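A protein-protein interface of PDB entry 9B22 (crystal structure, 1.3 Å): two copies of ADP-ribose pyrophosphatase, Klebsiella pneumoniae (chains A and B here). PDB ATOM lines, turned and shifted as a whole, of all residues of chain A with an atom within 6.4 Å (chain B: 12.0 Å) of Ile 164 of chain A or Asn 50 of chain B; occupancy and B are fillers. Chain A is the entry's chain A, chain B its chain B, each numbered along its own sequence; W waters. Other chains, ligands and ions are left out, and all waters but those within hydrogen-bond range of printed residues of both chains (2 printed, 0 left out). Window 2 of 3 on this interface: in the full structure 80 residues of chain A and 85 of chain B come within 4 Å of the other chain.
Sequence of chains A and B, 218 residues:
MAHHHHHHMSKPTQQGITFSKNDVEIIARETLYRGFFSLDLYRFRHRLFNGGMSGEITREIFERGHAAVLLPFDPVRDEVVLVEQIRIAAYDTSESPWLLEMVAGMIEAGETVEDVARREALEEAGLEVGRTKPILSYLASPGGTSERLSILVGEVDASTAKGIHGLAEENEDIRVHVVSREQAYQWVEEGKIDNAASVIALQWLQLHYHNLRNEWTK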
ATOM      1  N   GLU A 124      -1.286 -26.493   1.023  1.00  0.00           N
ATOM      2  CA  GLU A 124      -0.685 -26.362  -0.297  1.00  0.00           C
ATOM      3  C   GLU A 124      -0.631 -27.666  -1.075  1.00  0.00           C
ATOM      4  O   GLU A 124      -0.547 -27.634  -2.309  1.00  0.00           O
ATOM      5  CB  GLU A 124       0.726 -25.777  -0.174  1.00  0.00           C
ATOM      6  CG  GLU A 124       0.724 -24.383   0.439  1.00  0.00           C
ATOM      7  CD  GLU A 124       2.053 -23.629   0.345  1.00  0.00           C
ATOM      8  OE1 GLU A 124       3.109 -24.253   0.054  1.00  0.00           O
ATOM      9  OE2 GLU A 124       2.005 -22.393   0.598  1.00  0.00           O
ATOM     10  N   LYS A 162      -1.876 -35.404  -4.681  1.00  0.00           N
ATOM     11  CA  LYS A 162      -2.287 -35.042  -6.031  1.00  0.00           C
ATOM     12  C   LYS A 162      -3.198 -33.830  -5.954  1.00  0.00           C
ATOM     13  O   LYS A 162      -3.648 -33.432  -4.877  1.00  0.00           O
ATOM     14  CB  LYS A 162      -2.990 -36.204  -6.741  1.00  0.00           C
ATOM     15  CG  LYS A 162      -4.088 -36.846  -5.929  1.00  0.00           C
ATOM     16  CD  LYS A 162      -4.728 -38.014  -6.696  1.00  0.00           C
ATOM     17  CE  LYS A 162      -5.789 -38.727  -5.868  1.00  0.00           C
ATOM     18  NZ  LYS A 162      -6.791 -37.769  -5.314  1.00  0.00           N
ATOM     19  N   GLY A 163      -3.429 -33.231  -7.115  1.00  0.00           N
ATOM     20  CA  GLY A 163      -4.483 -32.261  -7.276  1.00  0.00           C
ATOM     21  C   GLY A 163      -4.012 -30.823  -7.198  1.00  0.00           C
ATOM     22  O   GLY A 163      -2.821 -30.503  -7.127  1.00  0.00           O
ATOM     23  N   ILE A 164      -5.014 -29.949  -7.198  1.00  0.00           N
ATOM     24  CA  ILE A 164      -4.849 -28.503  -7.182  1.00  0.00           C
ATOM     25  C   ILE A 164      -5.269 -28.012  -5.809  1.00  0.00           C
ATOM     26  O   ILE A 164      -6.340 -28.390  -5.310  1.00  0.00           O
ATOM     27  CB  ILE A 164      -5.717 -27.834  -8.263  1.00  0.00           C
ATOM     28  CG1 ILE A 164      -5.412 -28.436  -9.637  1.00  0.00           C
ATOM     29  CG2 ILE A 164      -5.513 -26.322  -8.244  1.00  0.00           C
ATOM     30  CD1 ILE A 164      -3.946 -28.506  -9.963  1.00  0.00           C
ATOM     31  N   HIS A 165      -4.429 -27.183  -5.206  1.00  0.00           N
ATOM     32  CA  HIS A 165      -4.638 -26.706  -3.846  1.00  0.00           C
ATOM     33  C   HIS A 165      -4.325 -25.220  -3.791  1.00  0.00           C
ATOM     34  O   HIS A 165      -4.237 -24.536  -4.817  1.00  0.00           O
ATOM     35  CB  HIS A 165      -3.772 -27.517  -2.874  1.00  0.00           C
ATOM     36  CG  HIS A 165      -4.029 -28.987  -2.941  1.00  0.00           C
ATOM     37  ND1 HIS A 165      -4.922 -29.626  -2.105  1.00  0.00           N
ATOM     38  CD2 HIS A 165      -3.537 -29.941  -3.770  1.00  0.00           C
ATOM     39  CE1 HIS A 165      -4.956 -30.913  -2.407  1.00  0.00           C
ATOM     40  NE2 HIS A 165      -4.125 -31.130  -3.410  1.00  0.00           N
ATOM     41  N   GLY A 166      -4.158 -24.714  -2.582  1.00  0.00           N
ATOM     42  CA  GLY A 166      -3.992 -23.292  -2.376  1.00  0.00           C
ATOM     43  C   GLY A 166      -5.301 -22.626  -1.991  1.00  0.00           C
ATOM     44  O   GLY A 166      -6.396 -23.087  -2.335  1.00  0.00           O
ATOM     45  N   ASP A 173      -2.820 -20.661  -6.230  1.00  0.00           N
ATOM     46  CA  ASP A 173      -3.199 -21.722  -7.159  1.00  0.00           C
ATOM     47  C   ASP A 173      -1.980 -22.627  -7.283  1.00  0.00           C
ATOM     48  O   ASP A 173      -0.950 -22.199  -7.803  1.00  0.00           O
ATOM     49  CB  ASP A 173      -3.585 -21.114  -8.509  1.00  0.00           C
ATOM     50  CG  ASP A 173      -4.151 -22.123  -9.473  1.00  0.00           C
ATOM     51  OD1 ASP A 173      -5.000 -22.939  -9.066  1.00  0.00           O
ATOM     52  OD2 ASP A 173      -3.763 -22.067 -10.659  1.00  0.00           O
ATOM     53  N   ILE A 174      -2.084 -23.860  -6.787  1.00  0.00           N
ATOM     54  CA  ILE A 174      -0.924 -24.722  -6.582  1.00  0.00           C
ATOM     55  C   ILE A 174      -1.235 -26.105  -7.136  1.00  0.00           C
ATOM     56  O   ILE A 174      -2.294 -26.662  -6.840  1.00  0.00           O
ATOM     57  CB  ILE A 174      -0.568 -24.808  -5.079  1.00  0.00           C
ATOM     58  CG1 ILE A 174      -0.287 -23.400  -4.512  1.00  0.00           C
ATOM     59  CG2 ILE A 174       0.621 -25.729  -4.868  1.00  0.00           C
ATOM     60  CD1 ILE A 174       0.094 -23.376  -3.013  1.00  0.00           C
ATOM     61  N   ARG A 175      -0.307 -26.665  -7.920  1.00  0.00           N
ATOM     62  CA  ARG A 175      -0.441 -28.011  -8.472  1.00  0.00           C
ATOM     63  C   ARG A 175       0.596 -28.938  -7.851  1.00  0.00           C
ATOM     64  O   ARG A 175       1.783 -28.605  -7.787  1.00  0.00           O
ATOM     65  CB  ARG A 175      -0.231 -28.004  -9.986  1.00  0.00           C
ATOM     66  CG  ARG A 175      -0.310 -29.380 -10.621  1.00  0.00           C
ATOM     67  CD  ARG A 175      -0.300 -29.317 -12.137  1.00  0.00           C
ATOM     68  NE  ARG A 175      -0.379 -30.661 -12.684  1.00  0.00           N
ATOM     69  CZ  ARG A 175      -0.308 -30.953 -13.977  1.00  0.00           C
ATOM     70  NH1 ARG A 175      -0.155 -30.009 -14.887  1.00  0.00           N
ATOM     71  NH2 ARG A 175      -0.395 -32.224 -14.361  1.00  0.00           N
ATOM     72  N   VAL A 176       0.161 -30.095  -7.416  1.00  0.00           N
ATOM     73  CA  VAL A 176       1.048 -31.074  -6.794  1.00  0.00           C
ATOM     74  C   VAL A 176       1.684 -31.956  -7.859  1.00  0.00           C
ATOM     75  O   VAL A 176       1.011 -32.425  -8.781  1.00  0.00           O
ATOM     76  CB  VAL A 176       0.255 -31.926  -5.787  1.00  0.00           C
ATOM     77  CG1 VAL A 176       1.069 -33.151  -5.368  1.00  0.00           C
ATOM     78  CG2 VAL A 176      -0.162 -31.084  -4.591  1.00  0.00           C
ATOM     79  N   GLY B  16       6.738 -32.073 -15.823  1.00  0.00           N
ATOM     80  CA  GLY B  16       7.298 -30.775 -15.456  1.00  0.00           C
ATOM     81  C   GLY B  16       6.244 -29.687 -15.330  1.00  0.00           C
ATOM     82  O   GLY B  16       5.047 -29.950 -15.187  1.00  0.00           O
ATOM     83  N   ILE B  17       6.705 -28.430 -15.389  1.00  0.00           N
ATOM     84  CA  ILE B  17       5.781 -27.313 -15.188  1.00  0.00           C
ATOM     85  C   ILE B  17       4.709 -27.277 -16.275  1.00  0.00           C
ATOM     86  O   ILE B  17       4.870 -27.807 -17.385  1.00  0.00           O
ATOM     87  CB  ILE B  17       6.483 -25.948 -15.075  1.00  0.00           C
ATOM     88  CG1 ILE B  17       7.298 -25.655 -16.334  1.00  0.00           C
ATOM     89  CG2 ILE B  17       7.335 -25.873 -13.799  1.00  0.00           C
ATOM     90  CD1 ILE B  17       7.746 -24.204 -16.423  1.00  0.00           C
ATOM     91  N   THR B  18       3.630 -26.563 -15.962  1.00  0.00           N
ATOM     92  CA  THR B  18       2.394 -26.581 -16.733  1.00  0.00           C
ATOM     93  C   THR B  18       2.261 -25.407 -17.702  1.00  0.00           C
ATOM     94  O   THR B  18       1.711 -25.585 -18.792  1.00  0.00           O
ATOM     95  CB  THR B  18       1.209 -26.583 -15.745  1.00  0.00           C
ATOM     96  OG1 THR B  18       1.319 -27.689 -14.825  1.00  0.00           O
ATOM     97  CG2 THR B  18      -0.116 -26.676 -16.462  1.00  0.00           C
ATOM     98  N   PHE B  19       2.780 -24.228 -17.364  1.00  0.00           N
ATOM     99  CA  PHE B  19       2.483 -22.984 -18.063  1.00  0.00           C
ATOM    100  C   PHE B  19       3.763 -22.225 -18.385  1.00  0.00           C
ATOM    101  O   PHE B  19       4.811 -22.467 -17.786  1.00  0.00           O
ATOM    102  CB  PHE B  19       1.599 -22.101 -17.182  1.00  0.00           C
ATOM    103  CG  PHE B  19       0.224 -22.649 -16.965  1.00  0.00           C
ATOM    104  CD1 PHE B  19      -0.619 -22.925 -18.032  1.00  0.00           C
ATOM    105  CD2 PHE B  19      -0.242 -22.863 -15.678  1.00  0.00           C
ATOM    106  CE1 PHE B  19      -1.912 -23.405 -17.816  1.00  0.00           C
ATOM    107  CE2 PHE B  19      -1.523 -23.354 -15.461  1.00  0.00           C
ATOM    108  CZ  PHE B  19      -2.353 -23.623 -16.529  1.00  0.00           C
ATOM    109  N   ASP B  23       1.242 -17.371 -20.573  1.00  0.00           N
ATOM    110  CA  ASP B  23       0.105 -17.583 -19.687  1.00  0.00           C
ATOM    111  C   ASP B  23      -0.009 -16.543 -18.584  1.00  0.00           C
ATOM    112  O   ASP B  23      -0.843 -16.693 -17.687  1.00  0.00           O
ATOM    113  CB  ASP B  23       0.214 -18.977 -19.083  1.00  0.00           C
ATOM    114  CG  ASP B  23       0.067 -20.059 -20.132  1.00  0.00           C
ATOM    115  OD1 ASP B  23      -0.987 -20.071 -20.788  1.00  0.00           O
ATOM    116  OD2 ASP B  23       0.981 -20.883 -20.312  1.00  0.00           O
ATOM    117  N   HIS B  46      -2.834 -14.272 -14.234  1.00  0.00           N
ATOM    118  CA  HIS B  46      -2.192 -15.482 -14.724  1.00  0.00           C
ATOM    119  C   HIS B  46      -3.194 -16.615 -14.872  1.00  0.00           C
ATOM    120  O   HIS B  46      -4.228 -16.653 -14.204  1.00  0.00           O
ATOM    121  CB  HIS B  46      -1.050 -15.945 -13.805  1.00  0.00           C
ATOM    122  CG  HIS B  46      -1.500 -16.324 -12.433  1.00  0.00           C
ATOM    123  ND1 HIS B  46      -1.891 -17.609 -12.111  1.00  0.00           N
ATOM    124  CD2 HIS B  46      -1.604 -15.598 -11.294  1.00  0.00           C
ATOM    125  CE1 HIS B  46      -2.210 -17.652 -10.827  1.00  0.00           C
ATOM    126  NE2 HIS B  46      -2.055 -16.447 -10.313  1.00  0.00           N
ATOM    127  N   ARG B  47      -2.847 -17.551 -15.761  1.00  0.00           N
ATOM    128  CA  ARG B  47      -3.702 -18.702 -16.011  1.00  0.00           C
ATOM    129  C   ARG B  47      -3.725 -19.604 -14.787  1.00  0.00           C
ATOM    130  O   ARG B  47      -2.730 -19.714 -14.061  1.00  0.00           O
ATOM    131  CB  ARG B  47      -3.238 -19.446 -17.268  1.00  0.00           C
ATOM    132  CG  ARG B  47      -4.159 -20.589 -17.699  1.00  0.00           C
ATOM    133  CD  ARG B  47      -4.085 -20.886 -19.209  1.00  0.00           C
ATOM    134  NE  ARG B  47      -4.980 -20.021 -19.960  1.00  0.00           N
ATOM    135  CZ  ARG B  47      -4.653 -18.877 -20.534  1.00  0.00           C
ATOM    136  NH1 ARG B  47      -3.399 -18.476 -20.634  1.00  0.00           N
ATOM    137  NH2 ARG B  47      -5.615 -18.118 -21.039  1.00  0.00           N
ATOM    138  N   LEU B  48      -4.871 -20.222 -14.557  1.00  0.00           N
ATOM    139  CA  LEU B  48      -5.145 -21.100 -13.432  1.00  0.00           C
ATOM    140  C   LEU B  48      -5.107 -22.549 -13.896  1.00  0.00           C
ATOM    141  O   LEU B  48      -5.485 -22.865 -15.029  1.00  0.00           O
ATOM    142  CB  LEU B  48      -6.533 -20.792 -12.849  1.00  0.00           C
ATOM    143  CG  LEU B  48      -6.709 -19.366 -12.341  1.00  0.00           C
ATOM    144  CD1 LEU B  48      -8.159 -19.124 -11.929  1.00  0.00           C
ATOM    145  CD2 LEU B  48      -5.757 -19.079 -11.189  1.00  0.00           C
ATOM    146  N   PHE B  49      -4.666 -23.429 -12.998  1.00  0.00           N
ATOM    147  CA  PHE B  49      -4.536 -24.843 -13.351  1.00  0.00           C
ATOM    148  C   PHE B  49      -5.852 -25.445 -13.833  1.00  0.00           C
ATOM    149  O   PHE B  49      -5.852 -26.318 -14.712  1.00  0.00           O
ATOM    150  CB  PHE B  49      -3.993 -25.641 -12.163  1.00  0.00           C
ATOM    151  CG  PHE B  49      -2.562 -25.331 -11.859  1.00  0.00           C
ATOM    152  CD1 PHE B  49      -1.582 -25.635 -12.779  1.00  0.00           C
ATOM    153  CD2 PHE B  49      -2.207 -24.703 -10.681  1.00  0.00           C
ATOM    154  CE1 PHE B  49      -0.266 -25.330 -12.528  1.00  0.00           C
ATOM    155  CE2 PHE B  49      -0.898 -24.385 -10.418  1.00  0.00           C
ATOM    156  CZ  PHE B  49       0.078 -24.704 -11.339  1.00  0.00           C
ATOM    157  N   ASN B  50      -6.977 -25.025 -13.255  1.00  0.00           N
ATOM    158  CA  ASN B  50      -8.275 -25.552 -13.665  1.00  0.00           C
ATOM    159  C   ASN B  50      -8.929 -24.745 -14.785  1.00  0.00           C
ATOM    160  O   ASN B  50     -10.092 -25.010 -15.133  1.00  0.00           O
ATOM    161  CB  ASN B  50      -9.207 -25.651 -12.455  1.00  0.00           C
ATOM    162  CG  ASN B  50      -8.818 -26.778 -11.518  1.00  0.00           C
ATOM    163  OD1 ASN B  50      -8.510 -27.887 -11.958  1.00  0.00           O
ATOM    164  ND2 ASN B  50      -8.818 -26.497 -10.223  1.00  0.00           N
ATOM    165  N   GLY B  51      -8.220 -23.792 -15.363  1.00  0.00           N
ATOM    166  CA  GLY B  51      -8.686 -23.070 -16.526  1.00  0.00           C
ATOM    167  C   GLY B  51      -9.013 -21.619 -16.226  1.00  0.00           C
ATOM    168  O   GLY B  51      -9.399 -21.251 -15.113  1.00  0.00           O
ATOM    169  N   GLY B  52      -8.888 -20.789 -17.246  1.00  0.00           N
ATOM    170  CA  GLY B  52      -9.192 -19.374 -17.117  1.00  0.00           C
ATOM    171  C   GLY B  52      -8.029 -18.610 -16.519  1.00  0.00           C
ATOM    172  O   GLY B  52      -6.973 -19.154 -16.217  1.00  0.00           O
ATOM    173  N   MET B  53      -8.258 -17.316 -16.308  1.00  0.00           N
ATOM    174  CA  MET B  53      -7.266 -16.427 -15.725  1.00  0.00           C
ATOM    175  C   MET B  53      -7.722 -15.953 -14.353  1.00  0.00           C
ATOM    176  O   MET B  53      -8.920 -15.833 -14.075  1.00  0.00           O
ATOM    177  CB  MET B  53      -7.048 -15.179 -16.588  1.00  0.00           C
ATOM    178  CG  MET B  53      -6.606 -15.431 -18.003  1.00  0.00           C
ATOM    179  SD  MET B  53      -4.906 -15.979 -18.066  1.00  0.00           S
ATOM    180  CE  MET B  53      -3.999 -14.441 -17.833  1.00  0.00           C
ATOM    181  N   SER B  54      -6.737 -15.672 -13.504  1.00  0.00           N
ATOM    182  CA  SER B  54      -6.990 -14.995 -12.247  1.00  0.00           C
ATOM    183  C   SER B  54      -7.528 -13.589 -12.506  1.00  0.00           C
ATOM    184  O   SER B  54      -7.414 -13.034 -13.608  1.00  0.00           O
ATOM    185  CB  SER B  54      -5.676 -14.890 -11.467  1.00  0.00           C
ATOM    186  OG  SER B  54      -4.785 -13.971 -12.079  1.00  0.00           O
HETATM  187  O   HOH W   1      -7.066 -23.727 -10.676  1.00  0.00           O
HETATM  188  O   HOH W   2      -1.481 -21.097 -11.923  1.00  0.00           O
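OD2 of Asp 173 of chain A lies within hydrogen-bond range of N of Phe 49 of chain B, at 2.9 Å.
OG1 of Thr 18 of chain B sits at hydrogen-bond distance from NH1 of Arg 175 of chain A (2.7 Å).
The backbone carbonyl oxygen (O) of Ile 174 of chain A is in hydrogen-bond range of the backbone NH (N) of His 165 of chain A (2.7 Å).
Ile 164 of chain A touches Phe 49 of chain B (CD1 to CB, 3.6 Å).
Ile 164 of chain A touches Asn 50 of chain B (CG2 to ND2, 3.9 Å).
Leu 48 of chain B touches Asp 173 of chain A.
C of Ile 174 of chain A touches CE2 of Phe 49 of chain B, 3.7 Å away.
CE2 of Phe 49 of chain B touches N of Arg 175 of chain A, 3.4 Å away.
Of chain B, only Phe 49 (3.6 Å) and Asn 50 (3.9 Å) come within 4 Å of Ile 164 of chain A.
Of chain A, only Ile 164 (3.9 Å) comes within 4 Å of Asn 50 of chain B.
No residue of chain B comes within 4 Å of Gly 163 of chain A.
No residue of chain B comes within 4 Å of Gly 166 of chain A.
Of chain B, only Phe 49 (3.7 Å) comes within 4 Å of Ile 174 of chain A.
Of chain B, only Thr 18 (2.7 Å) and Phe 49 (3.4 Å) come within 4 Å of Arg 175 of chain A.
No residue of chain B comes within 4 Å of Val 176 of chain A.
Printed residues of chain A within 4 Å of Leu 48 of chain B: Asp 173.
Printed residues of chain A within 4 Å of Thr 18 of chain B: Arg 175.
Printed residues of chain A within 4 Å of Phe 49 of chain B: Ile 164, Asp 173, Ile 174 and Arg 175.
The nearest residue of chain A that does not touch Asn 50 of chain B is Asp 173 of chain A (5.1 Å).
The nearest printed residue of chain A that does not touch Leu 48 of chain B is Ile 164 of chain A (6.8 Å).
Of the 14 printed residues of chain B, 4 touch a printed residue of chain A.
Printed residues of chain B that touch a printed residue of chain A: Thr 18, Leu 48, Phe 49 and Asn 50.
Of the 10 printed residues of chain A, 4 touch a printed residue of chain B.
Hydrophobic or aromatic side chains of chain A within 4 Å of the printed part of chain B: Ile 164.
Among the printed residues, 7 pairs touch across the chains.
Among the printed residues, no Asp or Glu carboxylate lies within 4 Å of a Lys or Arg side-chain nitrogen of the other chain.
No position is printed for both chains.
Water W1 lies within hydrogen-bond range of the side-chain carboxylate of Asp 173 of chain A, the backbone NH of Asn 50 of chain B and the backbone NH of Phe 49 of chain B.
Water W2 bridges the side-chain carboxylate (OD2) of Asp 173 of chain A (2.8 Å) and the backbone carbonyl oxygen (O) of Arg 47 of chain B (2.8 Å).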
